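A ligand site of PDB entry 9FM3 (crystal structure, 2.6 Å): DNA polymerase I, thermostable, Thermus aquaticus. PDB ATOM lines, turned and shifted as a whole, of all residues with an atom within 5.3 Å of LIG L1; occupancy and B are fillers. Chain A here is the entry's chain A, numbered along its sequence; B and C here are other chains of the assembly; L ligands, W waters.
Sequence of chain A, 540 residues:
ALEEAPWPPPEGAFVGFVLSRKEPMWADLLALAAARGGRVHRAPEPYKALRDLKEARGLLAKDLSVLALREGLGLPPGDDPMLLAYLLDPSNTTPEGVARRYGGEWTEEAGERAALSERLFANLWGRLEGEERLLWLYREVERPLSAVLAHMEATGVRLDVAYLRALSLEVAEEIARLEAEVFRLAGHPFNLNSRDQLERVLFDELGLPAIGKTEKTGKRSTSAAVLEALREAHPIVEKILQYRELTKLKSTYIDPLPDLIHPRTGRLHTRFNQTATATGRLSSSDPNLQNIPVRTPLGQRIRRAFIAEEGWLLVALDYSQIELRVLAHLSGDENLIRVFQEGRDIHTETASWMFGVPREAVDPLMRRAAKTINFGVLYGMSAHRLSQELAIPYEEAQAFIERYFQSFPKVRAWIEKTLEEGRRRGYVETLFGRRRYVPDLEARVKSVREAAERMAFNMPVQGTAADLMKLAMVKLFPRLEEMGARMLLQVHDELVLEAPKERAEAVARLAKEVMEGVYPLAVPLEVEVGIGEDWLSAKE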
ATOM      1  N   ARG A 281      11.053  27.815  -0.449  1.00  0.00           N
ATOM      2  CA  ARG A 281      10.033  27.073  -1.179  1.00  0.00           C
ATOM      3  C   ARG A 281       8.667  27.229  -0.496  1.00  0.00           C
ATOM      4  O   ARG A 281       8.563  27.491   0.708  1.00  0.00           O
ATOM      5  CB  ARG A 281      10.393  25.582  -1.254  1.00  0.00           C
ATOM      6  CG  ARG A 281      11.311  25.196  -2.395  1.00  0.00           C
ATOM      7  CD  ARG A 281      11.345  23.692  -2.574  1.00  0.00           C
ATOM      8  NE  ARG A 281      12.171  23.292  -3.705  1.00  0.00           N
ATOM      9  CZ  ARG A 281      12.284  22.040  -4.151  1.00  0.00           C
ATOM     10  NH1 ARG A 281      11.611  21.045  -3.589  1.00  0.00           N
ATOM     11  NH2 ARG A 281      13.077  21.788  -5.187  1.00  0.00           N
ATOM     12  N   GLN A 290       1.506  18.728  -3.511  1.00  0.00           N
ATOM     13  CA  GLN A 290       2.846  18.754  -4.084  1.00  0.00           C
ATOM     14  C   GLN A 290       3.540  17.398  -4.030  1.00  0.00           C
ATOM     15  O   GLN A 290       4.742  17.316  -4.338  1.00  0.00           O
ATOM     16  CB  GLN A 290       3.703  19.822  -3.387  1.00  0.00           C
ATOM     17  CG  GLN A 290       3.397  21.260  -3.817  1.00  0.00           C
ATOM     18  CD  GLN A 290       4.185  22.302  -3.030  1.00  0.00           C
ATOM     19  OE1 GLN A 290       4.811  22.005  -2.010  1.00  0.00           O
ATOM     20  NE2 GLN A 290       4.159  23.549  -3.511  1.00  0.00           N
ATOM     21  N   ILE A 292       1.684  14.354  -5.237  1.00  0.00           N
ATOM     22  CA  ILE A 292       0.826  13.398  -5.957  1.00  0.00           C
ATOM     23  C   ILE A 292       1.719  12.438  -6.744  1.00  0.00           C
ATOM     24  O   ILE A 292       2.599  12.896  -7.486  1.00  0.00           O
ATOM     25  CB  ILE A 292      -0.132  14.133  -6.888  1.00  0.00           C
ATOM     26  CG1 ILE A 292      -0.998  15.106  -6.103  1.00  0.00           C
ATOM     27  CG2 ILE A 292      -0.977  13.141  -7.668  1.00  0.00           C
ATOM     28  CD1 ILE A 292      -1.847  14.453  -5.053  1.00  0.00           C
ATOM     29  N   VAL A 294       3.583  10.030  -9.430  1.00  0.00           N
ATOM     30  CA  VAL A 294       3.833  10.300 -10.836  1.00  0.00           C
ATOM     31  C   VAL A 294       4.859   9.311 -11.389  1.00  0.00           C
ATOM     32  O   VAL A 294       5.065   9.226 -12.608  1.00  0.00           O
ATOM     33  CB  VAL A 294       4.286  11.754 -11.042  1.00  0.00           C
ATOM     34  CG1 VAL A 294       5.763  11.922 -10.662  1.00  0.00           C
ATOM     35  CG2 VAL A 294       4.021  12.226 -12.481  1.00  0.00           C
ATOM     36  N   ARG A 303      -2.822  10.808 -11.163  1.00  0.00           N
ATOM     37  CA  ARG A 303      -2.844  12.140 -11.775  1.00  0.00           C
ATOM     38  C   ARG A 303      -3.934  12.262 -12.828  1.00  0.00           C
ATOM     39  O   ARG A 303      -4.405  13.383 -13.086  1.00  0.00           O
ATOM     40  CB  ARG A 303      -1.475  12.467 -12.380  1.00  0.00           C
ATOM     41  CG  ARG A 303      -0.389  12.580 -11.330  1.00  0.00           C
ATOM     42  CD  ARG A 303       0.622  13.653 -11.651  1.00  0.00           C
ATOM     43  NE  ARG A 303       1.440  13.965 -10.488  1.00  0.00           N
ATOM     44  CZ  ARG A 303       2.400  14.878 -10.463  1.00  0.00           C
ATOM     45  NH1 ARG A 303       2.687  15.606 -11.525  1.00  0.00           N
ATOM     46  NH2 ARG A 303       3.087  15.066  -9.334  1.00  0.00           N
ATOM     47  N   ARG A 368      13.901   9.806 -15.030  1.00  0.00           N
ATOM     48  CA  ARG A 368      13.494  10.184 -13.685  1.00  0.00           C
ATOM     49  C   ARG A 368      14.413   9.570 -12.638  1.00  0.00           C
ATOM     50  O   ARG A 368      14.718  10.198 -11.622  1.00  0.00           O
ATOM     51  CB  ARG A 368      12.038   9.777 -13.424  1.00  0.00           C
ATOM     52  CG  ARG A 368      11.441  10.453 -12.203  1.00  0.00           C
ATOM     53  CD  ARG A 368      10.022   9.998 -11.919  1.00  0.00           C
ATOM     54  NE  ARG A 368       9.409  10.835 -10.896  1.00  0.00           N
ATOM     55  CZ  ARG A 368       9.642  10.723  -9.594  1.00  0.00           C
ATOM     56  NH1 ARG A 368      10.427   9.772  -9.110  1.00  0.00           N
ATOM     57  NH2 ARG A 368       9.080  11.586  -8.758  1.00  0.00           N
ATOM     58  N   VAL A 491       4.053  23.332  -8.041  1.00  0.00           N
ATOM     59  CA  VAL A 491       4.874  22.246  -7.518  1.00  0.00           C
ATOM     60  C   VAL A 491       6.337  22.627  -7.703  1.00  0.00           C
ATOM     61  O   VAL A 491       7.049  22.031  -8.519  1.00  0.00           O
ATOM     62  CB  VAL A 491       4.557  20.902  -8.195  1.00  0.00           C
ATOM     63  CG1 VAL A 491       5.072  19.762  -7.346  1.00  0.00           C
ATOM     64  CG2 VAL A 491       3.057  20.761  -8.409  1.00  0.00           C
ATOM     65  N   HIS A 492       6.776  23.645  -6.953  1.00  0.00           N
ATOM     66  CA  HIS A 492       8.163  24.069  -6.829  1.00  0.00           C
ATOM     67  C   HIS A 492       8.726  24.654  -8.124  1.00  0.00           C
ATOM     68  O   HIS A 492       9.119  25.825  -8.152  1.00  0.00           O
ATOM     69  CB  HIS A 492       9.011  22.898  -6.348  1.00  0.00           C
ATOM     70  CG  HIS A 492       8.478  22.269  -5.100  1.00  0.00           C
ATOM     71  ND1 HIS A 492       8.426  20.908  -4.909  1.00  0.00           N
ATOM     72  CD2 HIS A 492       7.942  22.827  -3.990  1.00  0.00           C
ATOM     73  CE1 HIS A 492       7.886  20.646  -3.729  1.00  0.00           C
ATOM     74  NE2 HIS A 492       7.587  21.796  -3.156  1.00  0.00           N
ATOM     75  N   ASP A 493       8.785  23.868  -9.190  1.00  0.00           N
ATOM     76  CA  ASP A 493       9.243  24.346 -10.487  1.00  0.00           C
ATOM     77  C   ASP A 493       8.185  24.171 -11.571  1.00  0.00           C
ATOM     78  O   ASP A 493       8.510  24.212 -12.761  1.00  0.00           O
ATOM     79  CB  ASP A 493      10.548  23.653 -10.897  1.00  0.00           C
ATOM     80  CG  ASP A 493      10.336  22.221 -11.354  1.00  0.00           C
ATOM     81  OD1 ASP A 493       9.521  21.499 -10.738  1.00  0.00           O
ATOM     82  OD2 ASP A 493      10.985  21.816 -12.341  1.00  0.00           O
ATOM     83  N   GLU A 494       6.927  23.973 -11.178  1.00  0.00           N
ATOM     84  CA  GLU A 494       5.862  23.613 -12.091  1.00  0.00           C
ATOM     85  C   GLU A 494       4.601  24.388 -11.746  1.00  0.00           C
ATOM     86  O   GLU A 494       4.239  24.489 -10.574  1.00  0.00           O
ATOM     87  CB  GLU A 494       5.587  22.093 -12.027  1.00  0.00           C
ATOM     88  CG  GLU A 494       4.406  21.615 -12.871  1.00  0.00           C
ATOM     89  CD  GLU A 494       4.110  20.136 -12.675  1.00  0.00           C
ATOM     90  OE1 GLU A 494       4.898  19.437 -11.995  1.00  0.00           O
ATOM     91  OE2 GLU A 494       3.078  19.653 -13.206  1.00  0.00           O
ATOM     92  N   LYS A 539       1.283  16.956 -18.536  1.00  0.00           N
ATOM     93  CA  LYS A 539       2.704  16.838 -18.249  1.00  0.00           C
ATOM     94  C   LYS A 539       3.467  16.137 -19.360  1.00  0.00           C
ATOM     95  O   LYS A 539       4.695  16.284 -19.446  1.00  0.00           O
ATOM     96  CB  LYS A 539       2.932  16.106 -16.918  1.00  0.00           C
ATOM     97  CG  LYS A 539       2.618  16.934 -15.689  1.00  0.00           C
ATOM     98  CD  LYS A 539       3.776  16.896 -14.682  1.00  0.00           C
ATOM     99  CE  LYS A 539       5.030  17.551 -15.253  1.00  0.00           C
ATOM    100  NZ  LYS A 539       6.171  17.540 -14.286  1.00  0.00           N
ATOM    101  P    DA B  11       6.344   9.436  -6.224  1.00  0.00           P
ATOM    102  OP1  DA B  11       5.777   8.982  -7.512  1.00  0.00           O
ATOM    103  OP2  DA B  11       7.619   8.879  -5.715  1.00  0.00           O
ATOM    104  O5'  DA B  11       6.508  11.021  -6.296  1.00  0.00           O
ATOM    105  C5'  DA B  11       5.428  11.808  -6.729  1.00  0.00           C
ATOM    106  C4'  DA B  11       5.591  13.230  -6.253  1.00  0.00           C
ATOM    107  O4'  DA B  11       5.967  13.227  -4.860  1.00  0.00           O
ATOM    108  C3'  DA B  11       6.685  14.008  -6.944  1.00  0.00           C
ATOM    109  O3'  DA B  11       6.169  14.625  -8.117  1.00  0.00           O
ATOM    110  C2'  DA B  11       7.080  15.048  -5.897  1.00  0.00           C
ATOM    111  C1'  DA B  11       6.776  14.350  -4.576  1.00  0.00           C
ATOM    112  N9   DA B  11       7.956  13.907  -3.846  1.00  0.00           N
ATOM    113  C8   DA B  11       8.526  12.655  -3.860  1.00  0.00           C
ATOM    114  N7   DA B  11       9.579  12.547  -3.066  1.00  0.00           N
ATOM    115  C5   DA B  11       9.696  13.805  -2.501  1.00  0.00           C
ATOM    116  C6   DA B  11      10.614  14.353  -1.571  1.00  0.00           C
ATOM    117  N6   DA B  11      11.620  13.663  -1.041  1.00  0.00           N
ATOM    118  N1   DA B  11      10.440  15.647  -1.217  1.00  0.00           N
ATOM    119  C2   DA B  11       9.421  16.339  -1.753  1.00  0.00           C
ATOM    120  N3   DA B  11       8.503  15.935  -2.626  1.00  0.00           N
ATOM    121  C4   DA B  11       8.696  14.649  -2.968  1.00  0.00           C
ATOM    122  P    DA C   4      24.135  10.039   2.353  1.00  0.00           P
ATOM    123  OP1  DA C   4      22.852   9.418   2.757  1.00  0.00           O
ATOM    124  OP2  DA C   4      25.183   9.220   1.713  1.00  0.00           O
ATOM    125  O5'  DA C   4      23.776  11.251   1.377  1.00  0.00           O
ATOM    126  C5'  DA C   4      22.738  12.147   1.749  1.00  0.00           C
ATOM    127  C4'  DA C   4      22.910  13.485   1.074  1.00  0.00           C
ATOM    128  O4'  DA C   4      22.832  13.306  -0.356  1.00  0.00           O
ATOM    129  C3'  DA C   4      21.855  14.502   1.425  1.00  0.00           C
ATOM    130  O3'  DA C   4      22.298  15.269   2.519  1.00  0.00           O
ATOM    131  C2'  DA C   4      21.743  15.348   0.159  1.00  0.00           C
ATOM    132  C1'  DA C   4      22.049  14.329  -0.935  1.00  0.00           C
ATOM    133  N9   DA C   4      20.867  13.710  -1.537  1.00  0.00           N
ATOM    134  C8   DA C   4      20.538  12.382  -1.536  1.00  0.00           C
ATOM    135  N7   DA C   4      19.429  12.108  -2.164  1.00  0.00           N
ATOM    136  C5   DA C   4      18.998  13.340  -2.641  1.00  0.00           C
ATOM    137  C6   DA C   4      17.877  13.727  -3.401  1.00  0.00           C
ATOM    138  N6   DA C   4      16.950  12.868  -3.826  1.00  0.00           N
ATOM    139  N1   DA C   4      17.757  15.038  -3.699  1.00  0.00           N
ATOM    140  C2   DA C   4      18.688  15.891  -3.269  1.00  0.00           C
ATOM    141  N3   DA C   4      19.781  15.644  -2.549  1.00  0.00           N
ATOM    142  C4   DA C   4      19.876  14.338  -2.263  1.00  0.00           C
ATOM    143  P    DG C   5      21.302  15.619   3.729  1.00  0.00           P
ATOM    144  OP1  DG C   5      22.137  16.158   4.823  1.00  0.00           O
ATOM    145  OP2  DG C   5      20.438  14.442   3.981  1.00  0.00           O
ATOM    146  O5'  DG C   5      20.405  16.807   3.154  1.00  0.00           O
ATOM    147  C5'  DG C   5      20.993  18.075   2.940  1.00  0.00           C
ATOM    148  C4'  DG C   5      20.116  18.924   2.049  1.00  0.00           C
ATOM    149  O4'  DG C   5      19.944  18.258   0.777  1.00  0.00           O
ATOM    150  C3'  DG C   5      18.706  19.140   2.540  1.00  0.00           C
ATOM    151  O3'  DG C   5      18.674  20.188   3.474  1.00  0.00           O
ATOM    152  C2'  DG C   5      18.002  19.528   1.241  1.00  0.00           C
ATOM    153  C1'  DG C   5      18.684  18.621   0.228  1.00  0.00           C
ATOM    154  N9   DG C   5      17.921  17.402  -0.058  1.00  0.00           N
ATOM    155  C8   DG C   5      18.236  16.117   0.307  1.00  0.00           C
ATOM    156  N7   DG C   5      17.366  15.235  -0.095  1.00  0.00           N
ATOM    157  C5   DG C   5      16.417  15.990  -0.777  1.00  0.00           C
ATOM    158  C6   DG C   5      15.229  15.577  -1.425  1.00  0.00           C
ATOM    159  O6   DG C   5      14.767  14.433  -1.545  1.00  0.00           O
ATOM    160  N1   DG C   5      14.539  16.666  -1.975  1.00  0.00           N
ATOM    161  C2   DG C   5      14.960  17.977  -1.907  1.00  0.00           C
ATOM    162  N2   DG C   5      14.169  18.879  -2.499  1.00  0.00           N
ATOM    163  N3   DG C   5      16.065  18.369  -1.295  1.00  0.00           N
ATOM    164  C4   DG C   5      16.745  17.323  -0.756  1.00  0.00           C
ATOM    165  P    DT C   6      17.404  20.332   4.446  1.00  0.00           P
ATOM    166  OP1  DT C   6      17.628  21.548   5.262  1.00  0.00           O
ATOM    167  OP2  DT C   6      17.151  19.015   5.065  1.00  0.00           O
ATOM    168  O5'  DT C   6      16.181  20.620   3.456  1.00  0.00           O
ATOM    169  C5'  DT C   6      16.072  21.875   2.813  1.00  0.00           C
ATOM    170  C4'  DT C   6      14.715  22.011   2.165  1.00  0.00           C
ATOM    171  O4'  DT C   6      14.609  21.101   1.052  1.00  0.00           O
ATOM    172  C3'  DT C   6      13.555  21.647   3.060  1.00  0.00           C
ATOM    173  O3'  DT C   6      13.212  22.726   3.912  1.00  0.00           O
ATOM    174  C2'  DT C   6      12.468  21.358   2.031  1.00  0.00           C
ATOM    175  C1'  DT C   6      13.256  20.653   0.931  1.00  0.00           C
ATOM    176  N1   DT C   6      13.217  19.158   1.023  1.00  0.00           N
ATOM    177  C2   DT C   6      12.196  18.478   0.389  1.00  0.00           C
ATOM    178  O2   DT C   6      11.336  19.036  -0.254  1.00  0.00           O
ATOM    179  N3   DT C   6      12.231  17.116   0.543  1.00  0.00           N
ATOM    180  C4   DT C   6      13.162  16.380   1.257  1.00  0.00           C
ATOM    181  O4   DT C   6      13.105  15.147   1.334  1.00  0.00           O
ATOM    182  C5   DT C   6      14.198  17.146   1.907  1.00  0.00           C
ATOM    183  C7   DT C   6      15.270  16.455   2.708  1.00  0.00           C
ATOM    184  C6   DT C   6      14.177  18.482   1.765  1.00  0.00           C
HETATM  185  N1  LIG L   1      10.794  16.925  -5.433  1.00  0.00           N
HETATM  186  C1  LIG L   1      11.882  17.023  -4.462  1.00  0.00           C
HETATM  187  N2  LIG L   1      12.555  15.854  -4.078  1.00  0.00           N
HETATM  188  C2  LIG L   1      12.175  14.679  -4.620  1.00  0.00           C
HETATM  189  C3  LIG L   1      11.101  14.556  -5.579  1.00  0.00           C
HETATM  190  C4  LIG L   1      10.454  15.697  -5.961  1.00  0.00           C
HETATM  191  O1  LIG L   1      12.168  18.122  -4.021  1.00  0.00           O
HETATM  192  N3  LIG L   1      12.864  13.571  -4.213  1.00  0.00           N
HETATM  193  C5  LIG L   1      10.033  18.128  -5.886  1.00  0.00           C
HETATM  194  C6  LIG L   1      10.780  18.888  -6.999  1.00  0.00           C
HETATM  195  C7  LIG L   1       9.766  19.000  -8.138  1.00  0.00           C
HETATM  196  C8  LIG L   1       8.445  18.508  -7.546  1.00  0.00           C
HETATM  197  O2  LIG L   1       8.751  17.750  -6.380  1.00  0.00           O
HETATM  198  C9  LIG L   1       7.663  17.569  -8.479  1.00  0.00           C
HETATM  199  O3  LIG L   1       8.260  16.307  -8.503  1.00  0.00           O
HETATM  200  P1  LIG L   1       7.435  15.000  -9.015  1.00  0.00           P
HETATM  201  O4  LIG L   1       6.344  15.555 -10.055  1.00  0.00           O
HETATM  202  O5  LIG L   1       8.298  13.970  -9.624  1.00  0.00           O
HETATM  203  C1  LG2 L   2      15.231  15.379  -6.186  1.00  0.00           C
HETATM  204  C2  LG2 L   2      15.910  17.705  -5.698  1.00  0.00           C
HETATM  205  C3  LG2 L   2      16.059  20.019  -7.976  1.00  0.00           C
HETATM  206  C4  LG2 L   2      15.286  20.138  -9.281  1.00  0.00           C
HETATM  207  O1  LG2 L   2      16.609  18.473  -5.050  1.00  0.00           O
HETATM  208  C5  LG2 L   2      12.769  20.300  -9.735  1.00  0.00           C
HETATM  209  C6  LG2 L   2      13.918  20.587  -8.790  1.00  0.00           C
HETATM  210  O2  LG2 L   2      15.387  14.197  -5.900  1.00  0.00           O
HETATM  211  C7  LG2 L   2      14.993  19.573  -6.973  1.00  0.00           C
HETATM  212  C8  LG2 L   2      14.263  17.246  -7.384  1.00  0.00           C
HETATM  213  C9  LG2 L   2      14.317  15.898  -7.195  1.00  0.00           C
HETATM  214  C10 LG2 L   2      13.459  15.020  -7.990  1.00  0.00           C
HETATM  215  C11 LG2 L   2      12.384  15.354  -8.785  1.00  0.00           C
HETATM  216  C12 LG2 L   2      11.753  14.270  -9.413  1.00  0.00           C
HETATM  217  C13 LG2 L   2      12.284  13.075  -9.143  1.00  0.00           C
HETATM  218  N1  LG2 L   2      15.956  16.346  -5.516  1.00  0.00           N
HETATM  219  N2  LG2 L   2      15.030  18.136  -6.680  1.00  0.00           N
HETATM  220  O3  LG2 L   2      15.881  21.136 -10.119  1.00  0.00           O
HETATM  221  O4  LG2 L   2      12.745  18.896 -10.039  1.00  0.00           O
HETATM  222  O5  LG2 L   2      11.223  19.442 -11.954  1.00  0.00           O
HETATM  223  O6  LG2 L   2      11.540  17.032 -11.200  1.00  0.00           O
HETATM  224  O7  LG2 L   2      13.409  18.276 -12.345  1.00  0.00           O
HETATM  225  O8  LG2 L   2      15.654  19.413 -12.345  1.00  0.00           O
HETATM  226  O9  LG2 L   2      13.610  20.635 -13.239  1.00  0.00           O
HETATM  227  O10 LG2 L   2      14.593  18.673 -14.479  1.00  0.00           O
HETATM  228  O11 LG2 L   2      13.535  18.962 -16.808  1.00  0.00           O
HETATM  229  O12 LG2 L   2      12.814  17.046 -15.337  1.00  0.00           O
HETATM  230  O13 LG2 L   2      12.068  19.394 -14.800  1.00  0.00           O
HETATM  231  O14 LG2 L   2      13.728  19.873  -7.552  1.00  0.00           O
HETATM  232  P1  LG2 L   2      12.105  18.392 -11.414  1.00  0.00           P
HETATM  233  P2  LG2 L   2      14.361  19.365 -13.051  1.00  0.00           P
HETATM  234  P3  LG2 L   2      13.142  18.522 -15.416  1.00  0.00           P
HETATM  235 SE1  LG2 L   2      13.719  13.175  -8.001  1.00  0.00          SE
HETATM  236  O   HOH W   1       8.115  19.380 -11.065  1.00  0.00           O
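Merely in contact with LIG L1: Val 294, Val 491, Asp 493 and DT 6 of chain C.
Hydrophobic or aromatic side chains that line LIG L1: Val 294, Val 491 and His 492.
Within 4 Å of LIG L1: Arg 281, Val 294, Arg 303, Arg 368, Val 491, His 492, Asp 493, DA 11 of chain B, DG 5 of chain C and DT 6 of chain C.
The nearest printed residue that does not touch LIG L1 is DA 4 of chain C (4.2 Å).
A nitrogen (N3) of LIG L1 is in hydrogen-bond range of an oxygen (O2) of LG2 L2, at 3.1 Å.
The guanidinium group (NH2) of Arg 303 lies within hydrogen-bond range of O3' of DA 11 of chain B.
The backbone NH of Val 294 lies within hydrogen-bond range of OP1 of DA 11 of chain B (3.1 Å).
ND1 of His 492 sits at hydrogen-bond distance from NH1 of Arg 281 (3.5 Å).
A ring nitrogen (NE2) of His 492 lies within hydrogen-bond range of the side-chain amide oxygen (OE1) of Gln 290.
NH2 of Arg 303 lies within hydrogen-bond range of O of Ile 292, 2.9 Å away.
Water W1 lies within hydrogen-bond range of OD1 of Asp 493 and OE1 of Glu 494.
O3' of DA 11 of chain B is bonded to a phosphorus (P1) of LIG L1 (1.6 Å).
A nitrogen (N3) of LIG L1 sits at hydrogen-bond distance from N6 of DA 11 of chain B (3.4 Å).
O6 of DG 5 of chain C is in hydrogen-bond range of a nitrogen (N3) of LIG L1 (3.4 Å).
An oxygen (O5) of LIG L1 is in salt-bridge range of the guanidinium group of Arg 368 (2.7 Å).
An oxygen (O1) of LIG L1 is in hydrogen-bond range of the guanidinium group of Arg 281 (3.0 Å).
A ring nitrogen (ND1) of His 492 sits close to an oxygen (O2) of LIG L1, at 3.5 Å.
The guanidinium group (NH2) of Arg 303 is in salt-bridge range of an oxygen (O4) of LIG L1 (3.4 Å).
An oxygen (O14) of LG2 L2 is in hydrogen-bond range of the guanidinium group of Arg 281 (3.1 Å).
N1 of DA 4 of chain C lies within hydrogen-bond range of a nitrogen (N1) of LG2 L2.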
